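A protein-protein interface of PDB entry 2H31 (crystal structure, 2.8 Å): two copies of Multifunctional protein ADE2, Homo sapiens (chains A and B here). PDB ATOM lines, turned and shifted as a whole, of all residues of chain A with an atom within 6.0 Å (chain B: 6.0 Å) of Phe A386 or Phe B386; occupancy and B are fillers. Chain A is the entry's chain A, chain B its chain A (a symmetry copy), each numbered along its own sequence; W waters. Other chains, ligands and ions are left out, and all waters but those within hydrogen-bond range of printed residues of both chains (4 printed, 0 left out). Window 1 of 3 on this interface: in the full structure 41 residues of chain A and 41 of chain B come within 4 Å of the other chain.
The backbone carbonyl oxygen (O) of Val A347 sits close to the side-chain sulfur (SG) of Cys A374, at 3.6 Å. The backbone carbonyl oxygen of Val A347 sits at hydrogen-bond distance from the backbone NH of Ser A375. The backbone carbonyl oxygen (O) of Val B347 lies close to the side-chain sulfur (SG) of Cys B374, 3.6 Å away. The backbone NH (N) of Ser B375 is in hydrogen-bond range of the backbone carbonyl oxygen (O) of Val B347, at 3.0 Å.
Among the printed residues, merely in contact across the chains: Pro A346 with Gln B389, Val A347 with Phe B386, Ile A348 with Phe B386, Gly A373 with Val B377, Gly A373 with Gly B382, Gly A373 with Gln B385, Gly A373 with Phe B386, Gly A373 with Gln B389, Cys A374 with Val B377, Ser A375 with Ser B375, Ser A375 with Val B377, Ser A375 with Phe B386, Val A377 with Gly B373, Val A377 with Cys B374, Val A377 with Ser B375, Gly A382 with Gly B373, Gln A385 with Gly B373, Phe A386 with Val B347, Phe A386 with Ile B348, Phe A386 with Gly B373, Phe A386 with Ser B375, Phe A386 with Phe B386, Gln A389 with Pro B346, Gln A389 with Gly B373 and Ile A390 with Ile B390.
Phe A386 touches just these residues of chain B: Val B347 (3.5 Å), Ile B348 (3.3 Å), Gly B373 (3.1 Å), Ser B375 (3.2 Å) and Phe B386 (3.1 Å). Of chain A, only Val A347 (3.5 Å), Ile A348 (3.3 Å), Gly A373 (3.1 Å), Ser A375 (3.2 Å) and Phe A386 (3.1 Å) come within 4 Å of Phe B386. Of the printed residues of chain A, Gln B385 touches Gly A373 (3.5 Å). Printed residues of chain B within 4 Å of Ser A375: Ser B375, Val B377 and Phe B386. Printed residues of chain B within 4 Å of Ile A390: Ile B390. Of the printed residues of chain A, Gly B382 touches Gly A373 (3.5 Å). Of the printed residues of chain A, Pro B346 touches Gln A389 (3.4 Å). Ala B388 touches none of the printed residues of chain A. The nearest residue of chain A that does not touch Phe B386 is Pro A346 (4.02 Å). The nearest printed residue of chain B that does not touch Val A377 is Val B347 (7.0 Å).
Of the 18 printed residues of chain A, 12 touch a printed residue of chain B. Hydrophobic or aromatic side chains of chain A that line the printed part of chain B: Pro A346, Ile A348, Val A377, Phe A386 and Ile A390. Along chain A the printed residues that touch a printed residue of chain B span positions 346 to 390. Among the printed residues, no Asp or Glu carboxylate lies within 4 Å of a Lys or Arg side-chain nitrogen of the other chain.
Val A347 touches Phe B386, and with the chains exchanged Phe A386 touches Val B347. Ile A348 touches Phe B386, and with the chains exchanged Phe A386 touches Ile B348. Gly A373 touches Phe B386, and with the chains exchanged Phe A386 touches Gly B373. Gly A373 touches Gln B389, and with the chains exchanged Gln A389 touches Gly B373. 18 positions are printed for both chains. Of the 25 pairs that touch across the chains among the printed residues, 25 have their exchanged pair printed and touching as well.
Water W4 lies within hydrogen-bond range of OE1 of Gln B389 (2.8 Å) and N of Val A347 (3.1 Å). Water W3 lies within hydrogen-bond range of OE1 of Gln A389 and N of Val B347. Water W1 lies within hydrogen-bond range of the backbone NH (N) of Gly B373, the side-chain amide nitrogen (NE2) of Gln A389 and the side-chain amide oxygen (OE1) of Gln A385. Water W2 lies within hydrogen-bond range of N of Gly A373 (2.9 Å), NE2 of Gln B389 (3.0 Å) and OE1 of Gln B385 (3.4 Å).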
ATOM      1  N   PRO A 346     -20.058   4.866  28.237  1.00  0.00           N
ATOM      2  CA  PRO A 346     -18.764   4.183  28.342  1.00  0.00           C
ATOM      3  C   PRO A 346     -17.789   4.565  27.232  1.00  0.00           C
ATOM      4  O   PRO A 346     -18.198   4.905  26.120  1.00  0.00           O
ATOM      5  CB  PRO A 346     -19.155   2.701  28.291  1.00  0.00           C
ATOM      6  CG  PRO A 346     -20.375   2.690  27.449  1.00  0.00           C
ATOM      7  CD  PRO A 346     -21.140   3.894  27.980  1.00  0.00           C
ATOM      8  N   VAL A 347     -16.498   4.529  27.544  1.00  0.00           N
ATOM      9  CA  VAL A 347     -15.477   4.829  26.546  1.00  0.00           C
ATOM     10  C   VAL A 347     -14.321   3.815  26.612  1.00  0.00           C
ATOM     11  O   VAL A 347     -13.645   3.674  27.640  1.00  0.00           O
ATOM     12  CB  VAL A 347     -14.931   6.253  26.721  1.00  0.00           C
ATOM     13  CG1 VAL A 347     -13.721   6.446  25.866  1.00  0.00           C
ATOM     14  CG2 VAL A 347     -15.970   7.254  26.306  1.00  0.00           C
ATOM     15  N   ILE A 348     -14.118   3.097  25.511  1.00  0.00           N
ATOM     16  CA  ILE A 348     -13.048   2.105  25.404  1.00  0.00           C
ATOM     17  C   ILE A 348     -11.902   2.678  24.576  1.00  0.00           C
ATOM     18  O   ILE A 348     -12.119   3.219  23.492  1.00  0.00           O
ATOM     19  CB  ILE A 348     -13.469   0.835  24.625  1.00  0.00           C
ATOM     20  CG1 ILE A 348     -14.858   0.354  25.036  1.00  0.00           C
ATOM     21  CG2 ILE A 348     -12.448  -0.248  24.855  1.00  0.00           C
ATOM     22  CD1 ILE A 348     -14.939  -0.189  26.432  1.00  0.00           C
ATOM     23  N   GLY A 373     -13.379   6.874  33.838  1.00  0.00           N
ATOM     24  CA  GLY A 373     -13.731   5.467  33.815  1.00  0.00           C
ATOM     25  C   GLY A 373     -13.137   4.725  32.637  1.00  0.00           C
ATOM     26  O   GLY A 373     -13.146   3.491  32.601  1.00  0.00           O
ATOM     27  N   CYS A 374     -12.619   5.488  31.682  1.00  0.00           N
ATOM     28  CA  CYS A 374     -12.032   4.957  30.461  1.00  0.00           C
ATOM     29  C   CYS A 374     -11.347   3.598  30.609  1.00  0.00           C
ATOM     30  O   CYS A 374     -10.444   3.422  31.439  1.00  0.00           O
ATOM     31  CB  CYS A 374     -11.040   5.973  29.901  1.00  0.00           C
ATOM     32  SG  CYS A 374     -10.725   5.761  28.150  1.00  0.00           S
ATOM     33  N   SER A 375     -11.768   2.632  29.797  1.00  0.00           N
ATOM     34  CA  SER A 375     -11.175   1.303  29.863  1.00  0.00           C
ATOM     35  C   SER A 375     -10.361   1.035  28.624  1.00  0.00           C
ATOM     36  O   SER A 375     -10.612   1.607  27.573  1.00  0.00           O
ATOM     37  CB  SER A 375     -12.250   0.223  29.975  1.00  0.00           C
ATOM     38  OG  SER A 375     -12.873   0.011  28.722  1.00  0.00           O
ATOM     39  N   VAL A 377      -8.729  -1.871  25.850  1.00  0.00           N
ATOM     40  CA  VAL A 377      -8.843  -3.213  25.260  1.00  0.00           C
ATOM     41  C   VAL A 377      -7.991  -3.207  24.005  1.00  0.00           C
ATOM     42  O   VAL A 377      -8.305  -2.508  23.035  1.00  0.00           O
ATOM     43  CB  VAL A 377     -10.277  -3.602  24.849  1.00  0.00           C
ATOM     44  CG1 VAL A 377     -10.240  -4.887  24.079  1.00  0.00           C
ATOM     45  CG2 VAL A 377     -11.143  -3.812  26.066  1.00  0.00           C
ATOM     46  N   GLU A 381     -11.160  -6.656  17.537  1.00  0.00           N
ATOM     47  CA  GLU A 381     -12.414  -7.396  17.625  1.00  0.00           C
ATOM     48  C   GLU A 381     -12.775  -7.527  19.094  1.00  0.00           C
ATOM     49  O   GLU A 381     -13.942  -7.479  19.469  1.00  0.00           O
ATOM     50  CB  GLU A 381     -12.304  -8.779  16.961  1.00  0.00           C
ATOM     51  CG  GLU A 381     -10.922  -9.399  16.984  1.00  0.00           C
ATOM     52  CD  GLU A 381      -9.954  -8.740  16.012  1.00  0.00           C
ATOM     53  OE1 GLU A 381      -8.767  -8.573  16.379  1.00  0.00           O
ATOM     54  OE2 GLU A 381     -10.377  -8.407  14.880  1.00  0.00           O
ATOM     55  N   GLY A 382     -11.756  -7.674  19.930  1.00  0.00           N
ATOM     56  CA  GLY A 382     -11.999  -7.781  21.355  1.00  0.00           C
ATOM     57  C   GLY A 382     -12.744  -6.563  21.885  1.00  0.00           C
ATOM     58  O   GLY A 382     -13.594  -6.682  22.751  1.00  0.00           O
ATOM     59  N   SER A 383     -12.445  -5.379  21.374  1.00  0.00           N
ATOM     60  CA  SER A 383     -13.141  -4.212  21.877  1.00  0.00           C
ATOM     61  C   SER A 383     -14.598  -4.243  21.432  1.00  0.00           C
ATOM     62  O   SER A 383     -15.481  -3.822  22.174  1.00  0.00           O
ATOM     63  CB  SER A 383     -12.443  -2.918  21.430  1.00  0.00           C
ATOM     64  OG  SER A 383     -12.527  -2.710  20.045  1.00  0.00           O
ATOM     65  N   ALA A 384     -14.851  -4.746  20.231  1.00  0.00           N
ATOM     66  CA  ALA A 384     -16.223  -4.845  19.735  1.00  0.00           C
ATOM     67  C   ALA A 384     -16.985  -5.839  20.635  1.00  0.00           C
ATOM     68  O   ALA A 384     -18.130  -5.607  21.035  1.00  0.00           O
ATOM     69  CB  ALA A 384     -16.226  -5.325  18.282  1.00  0.00           C
ATOM     70  N   GLN A 385     -16.323  -6.935  20.976  1.00  0.00           N
ATOM     71  CA  GLN A 385     -16.927  -7.924  21.834  1.00  0.00           C
ATOM     72  C   GLN A 385     -17.291  -7.302  23.178  1.00  0.00           C
ATOM     73  O   GLN A 385     -18.399  -7.502  23.686  1.00  0.00           O
ATOM     74  CB  GLN A 385     -15.964  -9.075  22.047  1.00  0.00           C
ATOM     75  CG  GLN A 385     -16.568 -10.252  22.790  1.00  0.00           C
ATOM     76  CD  GLN A 385     -15.667 -11.478  22.730  1.00  0.00           C
ATOM     77  OE1 GLN A 385     -16.032 -12.549  23.204  1.00  0.00           O
ATOM     78  NE2 GLN A 385     -14.480 -11.318  22.145  1.00  0.00           N
ATOM     79  N   PHE A 386     -16.371  -6.542  23.763  1.00  0.00           N
ATOM     80  CA  PHE A 386     -16.667  -5.928  25.048  1.00  0.00           C
ATOM     81  C   PHE A 386     -17.904  -5.043  24.891  1.00  0.00           C
ATOM     82  O   PHE A 386     -18.834  -5.106  25.705  1.00  0.00           O
ATOM     83  CB  PHE A 386     -15.483  -5.102  25.559  1.00  0.00           C
ATOM     84  CG  PHE A 386     -15.629  -4.662  26.998  1.00  0.00           C
ATOM     85  CD1 PHE A 386     -15.434  -5.567  28.041  1.00  0.00           C
ATOM     86  CD2 PHE A 386     -16.010  -3.351  27.308  1.00  0.00           C
ATOM     87  CE1 PHE A 386     -15.620  -5.178  29.375  1.00  0.00           C
ATOM     88  CE2 PHE A 386     -16.196  -2.958  28.631  1.00  0.00           C
ATOM     89  CZ  PHE A 386     -16.001  -3.877  29.666  1.00  0.00           C
ATOM     90  N   ALA A 387     -17.926  -4.226  23.839  1.00  0.00           N
ATOM     91  CA  ALA A 387     -19.068  -3.346  23.591  1.00  0.00           C
ATOM     92  C   ALA A 387     -20.349  -4.179  23.527  1.00  0.00           C
ATOM     93  O   ALA A 387     -21.366  -3.815  24.109  1.00  0.00           O
ATOM     94  CB  ALA A 387     -18.866  -2.576  22.290  1.00  0.00           C
ATOM     95  N   ALA A 388     -20.285  -5.303  22.815  1.00  0.00           N
ATOM     96  CA  ALA A 388     -21.431  -6.195  22.696  1.00  0.00           C
ATOM     97  C   ALA A 388     -21.877  -6.614  24.088  1.00  0.00           C
ATOM     98  O   ALA A 388     -23.053  -6.507  24.408  1.00  0.00           O
ATOM     99  CB  ALA A 388     -21.074  -7.426  21.868  1.00  0.00           C
ATOM    100  N   GLN A 389     -20.942  -7.084  24.917  1.00  0.00           N
ATOM    101  CA  GLN A 389     -21.279  -7.519  26.277  1.00  0.00           C
ATOM    102  C   GLN A 389     -21.889  -6.387  27.094  1.00  0.00           C
ATOM    103  O   GLN A 389     -22.679  -6.632  28.000  1.00  0.00           O
ATOM    104  CB  GLN A 389     -20.041  -8.075  26.990  1.00  0.00           C
ATOM    105  CG  GLN A 389     -19.391  -9.220  26.250  1.00  0.00           C
ATOM    106  CD  GLN A 389     -17.998  -9.519  26.758  1.00  0.00           C
ATOM    107  OE1 GLN A 389     -17.264  -8.611  27.158  1.00  0.00           O
ATOM    108  NE2 GLN A 389     -17.614 -10.793  26.728  1.00  0.00           N
ATOM    109  N   ILE A 390     -21.515  -5.147  26.777  1.00  0.00           N
ATOM    110  CA  ILE A 390     -22.087  -3.988  27.468  1.00  0.00           C
ATOM    111  C   ILE A 390     -23.568  -3.895  27.063  1.00  0.00           C
ATOM    112  O   ILE A 390     -24.457  -3.904  27.905  1.00  0.00           O
ATOM    113  CB  ILE A 390     -21.383  -2.661  27.075  1.00  0.00           C
ATOM    114  CG1 ILE A 390     -19.973  -2.617  27.646  1.00  0.00           C
ATOM    115  CG2 ILE A 390     -22.166  -1.478  27.607  1.00  0.00           C
ATOM    116  CD1 ILE A 390     -19.228  -1.325  27.341  1.00  0.00           C
ATOM    117  N   PHE A 391     -23.822  -3.815  25.762  1.00  0.00           N
ATOM    118  CA  PHE A 391     -25.181  -3.734  25.252  1.00  0.00           C
ATOM    119  C   PHE A 391     -25.974  -5.003  25.569  1.00  0.00           C
ATOM    120  O   PHE A 391     -27.187  -4.952  25.762  1.00  0.00           O
ATOM    121  CB  PHE A 391     -25.157  -3.503  23.747  1.00  0.00           C
ATOM    122  CG  PHE A 391     -24.730  -2.130  23.362  1.00  0.00           C
ATOM    123  CD1 PHE A 391     -23.664  -1.938  22.497  1.00  0.00           C
ATOM    124  CD2 PHE A 391     -25.421  -1.017  23.836  1.00  0.00           C
ATOM    125  CE1 PHE A 391     -23.292  -0.645  22.100  1.00  0.00           C
ATOM    126  CE2 PHE A 391     -25.055   0.281  23.446  1.00  0.00           C
ATOM    127  CZ  PHE A 391     -23.990   0.466  22.575  1.00  0.00           C
ATOM    128  N   PRO B 346     -20.205  -8.299  30.796  1.00  0.00           N
ATOM    129  CA  PRO B 346     -18.897  -7.638  30.728  1.00  0.00           C
ATOM    130  C   PRO B 346     -17.961  -8.036  31.865  1.00  0.00           C
ATOM    131  O   PRO B 346     -18.407  -8.369  32.965  1.00  0.00           O
ATOM    132  CB  PRO B 346     -19.265  -6.149  30.768  1.00  0.00           C
ATOM    133  CG  PRO B 346     -20.508  -6.117  31.575  1.00  0.00           C
ATOM    134  CD  PRO B 346     -21.277  -7.309  31.022  1.00  0.00           C
ATOM    135  N   VAL B 347     -16.661  -8.021  31.591  1.00  0.00           N
ATOM    136  CA  VAL B 347     -15.674  -8.339  32.617  1.00  0.00           C
ATOM    137  C   VAL B 347     -14.499  -7.344  32.584  1.00  0.00           C
ATOM    138  O   VAL B 347     -13.792  -7.214  31.576  1.00  0.00           O
ATOM    139  CB  VAL B 347     -15.147  -9.771  32.457  1.00  0.00           C
ATOM    140  CG1 VAL B 347     -13.966  -9.985  33.346  1.00  0.00           C
ATOM    141  CG2 VAL B 347     -16.214 -10.754  32.842  1.00  0.00           C
ATOM    142  N   ILE B 348     -14.316  -6.629  33.690  1.00  0.00           N
ATOM    143  CA  ILE B 348     -13.233  -5.655  33.828  1.00  0.00           C
ATOM    144  C   ILE B 348     -12.121  -6.247  34.688  1.00  0.00           C
ATOM    145  O   ILE B 348     -12.378  -6.784  35.765  1.00  0.00           O
ATOM    146  CB  ILE B 348     -13.655  -4.378  34.595  1.00  0.00           C
ATOM    147  CG1 ILE B 348     -15.024  -3.874  34.145  1.00  0.00           C
ATOM    148  CG2 ILE B 348     -12.610  -3.312  34.395  1.00  0.00           C
ATOM    149  CD1 ILE B 348     -15.056  -3.329  32.747  1.00  0.00           C
ATOM    150  N   GLY B 373     -13.404 -10.419  25.387  1.00  0.00           N
ATOM    151  CA  GLY B 373     -13.732  -9.007  25.400  1.00  0.00           C
ATOM    152  C   GLY B 373     -13.160  -8.275  26.595  1.00  0.00           C
ATOM    153  O   GLY B 373     -13.149  -7.041  26.631  1.00  0.00           O
ATOM    154  N   CYS B 374     -12.682  -9.047  27.564  1.00  0.00           N
ATOM    155  CA  CYS B 374     -12.122  -8.525  28.801  1.00  0.00           C
ATOM    156  C   CYS B 374     -11.410  -7.178  28.673  1.00  0.00           C
ATOM    157  O   CYS B 374     -10.481  -7.017  27.869  1.00  0.00           O
ATOM    158  CB  CYS B 374     -11.163  -9.557  29.389  1.00  0.00           C
ATOM    159  SG  CYS B 374     -10.895  -9.350  31.149  1.00  0.00           S
ATOM    160  N   SER B 375     -11.838  -6.205  29.473  1.00  0.00           N
ATOM    161  CA  SER B 375     -11.221  -4.885  29.424  1.00  0.00           C
ATOM    162  C   SER B 375     -10.438  -4.631  30.686  1.00  0.00           C
ATOM    163  O   SER B 375     -10.728  -5.199  31.729  1.00  0.00           O
ATOM    164  CB  SER B 375     -12.273  -3.788  29.283  1.00  0.00           C
ATOM    165  OG  SER B 375     -12.929  -3.565  30.517  1.00  0.00           O
ATOM    166  N   VAL B 377      -8.837  -1.752  33.506  1.00  0.00           N
ATOM    167  CA  VAL B 377      -8.946  -0.409  34.093  1.00  0.00           C
ATOM    168  C   VAL B 377      -8.130  -0.428  35.372  1.00  0.00           C
ATOM    169  O   VAL B 377      -8.483  -1.121  36.332  1.00  0.00           O
ATOM    170  CB  VAL B 377     -10.383   0.005  34.463  1.00  0.00           C
ATOM    171  CG1 VAL B 377     -10.347   1.289  35.234  1.00  0.00           C
ATOM    172  CG2 VAL B 377     -11.211   0.229  33.222  1.00  0.00           C
ATOM    173  N   GLU B 381     -11.423   3.074  41.748  1.00  0.00           N
ATOM    174  CA  GLU B 381     -12.662   3.836  41.625  1.00  0.00           C
ATOM    175  C   GLU B 381     -12.978   3.973  40.146  1.00  0.00           C
ATOM    176  O   GLU B 381     -14.135   3.944  39.737  1.00  0.00           O
ATOM    177  CB  GLU B 381     -12.548   5.217  42.292  1.00  0.00           C
ATOM    178  CG  GLU B 381     -11.155   5.813  42.308  1.00  0.00           C
ATOM    179  CD  GLU B 381     -10.226   5.139  43.307  1.00  0.00           C
ATOM    180  OE1 GLU B 381      -9.032   4.952  42.974  1.00  0.00           O
ATOM    181  OE2 GLU B 381     -10.687   4.813  44.426  1.00  0.00           O
ATOM    182  N   GLY B 382     -11.934   4.102  39.339  1.00  0.00           N
ATOM    183  CA  GLY B 382     -12.135   4.212  37.908  1.00  0.00           C
ATOM    184  C   GLY B 382     -12.884   3.008  37.357  1.00  0.00           C
ATOM    185  O   GLY B 382     -13.707   3.141  36.467  1.00  0.00           O
ATOM    186  N   SER B 383     -12.620   1.818  37.875  1.00  0.00           N
ATOM    187  CA  SER B 383     -13.321   0.664  37.352  1.00  0.00           C
ATOM    188  C   SER B 383     -14.789   0.719  37.756  1.00  0.00           C
ATOM    189  O   SER B 383     -15.658   0.313  36.989  1.00  0.00           O
ATOM    190  CB  SER B 383     -12.657  -0.642  37.819  1.00  0.00           C
ATOM    191  OG  SER B 383     -12.785  -0.848  39.201  1.00  0.00           O
ATOM    192  N   ALA B 384     -15.068   1.227  38.949  1.00  0.00           N
ATOM    193  CA  ALA B 384     -16.452   1.349  39.406  1.00  0.00           C
ATOM    194  C   ALA B 384     -17.171   2.355  38.485  1.00  0.00           C
ATOM    195  O   ALA B 384     -18.307   2.143  38.052  1.00  0.00           O
ATOM    196  CB  ALA B 384     -16.487   1.829  40.858  1.00  0.00           C
ATOM    197  N   GLN B 385     -16.481   3.440  38.163  1.00  0.00           N
ATOM    198  CA  GLN B 385     -17.043   4.438  37.288  1.00  0.00           C
ATOM    199  C   GLN B 385     -17.380   3.822  35.935  1.00  0.00           C
ATOM    200  O   GLN B 385     -18.469   4.041  35.395  1.00  0.00           O
ATOM    201  CB  GLN B 385     -16.055   5.574  37.103  1.00  0.00           C
ATOM    202  CG  GLN B 385     -16.618   6.760  36.344  1.00  0.00           C
ATOM    203  CD  GLN B 385     -15.699   7.971  36.429  1.00  0.00           C
ATOM    204  OE1 GLN B 385     -16.032   9.048  35.946  1.00  0.00           O
ATOM    205  NE2 GLN B 385     -14.531   7.791  37.048  1.00  0.00           N
ATOM    206  N   PHE B 386     -16.456   3.047  35.376  1.00  0.00           N
ATOM    207  CA  PHE B 386     -16.726   2.438  34.083  1.00  0.00           C
ATOM    208  C   PHE B 386     -17.982   1.573  34.204  1.00  0.00           C
ATOM    209  O   PHE B 386     -18.887   1.652  33.364  1.00  0.00           O
ATOM    210  CB  PHE B 386     -15.542   1.592  33.606  1.00  0.00           C
ATOM    211  CG  PHE B 386     -15.654   1.154  32.163  1.00  0.00           C
ATOM    212  CD1 PHE B 386     -15.414   2.055  31.126  1.00  0.00           C
ATOM    213  CD2 PHE B 386     -16.048  -0.150  31.842  1.00  0.00           C
ATOM    214  CE1 PHE B 386     -15.568   1.669  29.787  1.00  0.00           C
ATOM    215  CE2 PHE B 386     -16.202  -0.541  30.514  1.00  0.00           C
ATOM    216  CZ  PHE B 386     -15.963   0.375  29.486  1.00  0.00           C
ATOM    217  N   ALA B 387     -18.047   0.758  35.255  1.00  0.00           N
ATOM    218  CA  ALA B 387     -19.210  -0.104  35.470  1.00  0.00           C
ATOM    219  C   ALA B 387     -20.478   0.751  35.498  1.00  0.00           C
ATOM    220  O   ALA B 387     -21.484   0.404  34.887  1.00  0.00           O
ATOM    221  CB  ALA B 387     -19.059  -0.876  36.776  1.00  0.00           C
ATOM    222  N   ALA B 388     -20.416   1.874  36.211  1.00  0.00           N
ATOM    223  CA  ALA B 388     -21.549   2.785  36.298  1.00  0.00           C
ATOM    224  C   ALA B 388     -21.949   3.211  34.894  1.00  0.00           C
ATOM    225  O   ALA B 388     -23.116   3.124  34.541  1.00  0.00           O
ATOM    226  CB  ALA B 388     -21.195   4.010  37.136  1.00  0.00           C
ATOM    227  N   GLN B 389     -20.983   3.665  34.093  1.00  0.00           N
ATOM    228  CA  GLN B 389     -21.273   4.106  32.724  1.00  0.00           C
ATOM    229  C   GLN B 389     -21.879   2.983  31.889  1.00  0.00           C
ATOM    230  O   GLN B 389     -22.638   3.242  30.960  1.00  0.00           O
ATOM    231  CB  GLN B 389     -20.006   4.641  32.046  1.00  0.00           C
ATOM    232  CG  GLN B 389     -19.358   5.775  32.805  1.00  0.00           C
ATOM    233  CD  GLN B 389     -17.946   6.050  32.337  1.00  0.00           C
ATOM    234  OE1 GLN B 389     -17.217   5.130  31.957  1.00  0.00           O
ATOM    235  NE2 GLN B 389     -17.542   7.317  32.377  1.00  0.00           N
ATOM    236  N   ILE B 390     -21.535   1.737  32.216  1.00  0.00           N
ATOM    237  CA  ILE B 390     -22.106   0.589  31.509  1.00  0.00           C
ATOM    238  C   ILE B 390     -23.600   0.520  31.872  1.00  0.00           C
ATOM    239  O   ILE B 390     -24.464   0.544  31.005  1.00  0.00           O
ATOM    240  CB  ILE B 390     -21.436  -0.750  31.921  1.00  0.00           C
ATOM    241  CG1 ILE B 390     -20.012  -0.818  31.391  1.00  0.00           C
ATOM    242  CG2 ILE B 390     -22.224  -1.920  31.367  1.00  0.00           C
ATOM    243  CD1 ILE B 390     -19.298  -2.123  31.717  1.00  0.00           C
ATOM    244  N   PHE B 391     -23.891   0.445  33.164  1.00  0.00           N
ATOM    245  CA  PHE B 391     -25.266   0.387  33.636  1.00  0.00           C
ATOM    246  C   PHE B 391     -26.029   1.669  33.297  1.00  0.00           C
ATOM    247  O   PHE B 391     -27.236   1.639  33.069  1.00  0.00           O
ATOM    248  CB  PHE B 391     -25.289   0.156  35.140  1.00  0.00           C
ATOM    249  CG  PHE B 391     -24.896  -1.224  35.537  1.00  0.00           C
ATOM    250  CD1 PHE B 391     -23.858  -1.434  36.432  1.00  0.00           C
ATOM    251  CD2 PHE B 391     -25.592  -2.325  35.043  1.00  0.00           C
ATOM    252  CE1 PHE B 391     -23.519  -2.733  36.840  1.00  0.00           C
ATOM    253  CE2 PHE B 391     -25.259  -3.630  35.443  1.00  0.00           C
ATOM    254  CZ  PHE B 391     -24.222  -3.832  36.345  1.00  0.00           C
HETATM  255  O   HOH W   1     -15.141 -12.471  26.467  1.00  0.00           O
HETATM  256  O   HOH W   2     -15.050   8.954  32.709  1.00  0.00           O
HETATM  257  O   HOH W   3     -15.891  -9.809  29.238  1.00  0.00           O
HETATM  258  O   HOH W   4     -15.765   6.304  29.917  1.00  0.00           O
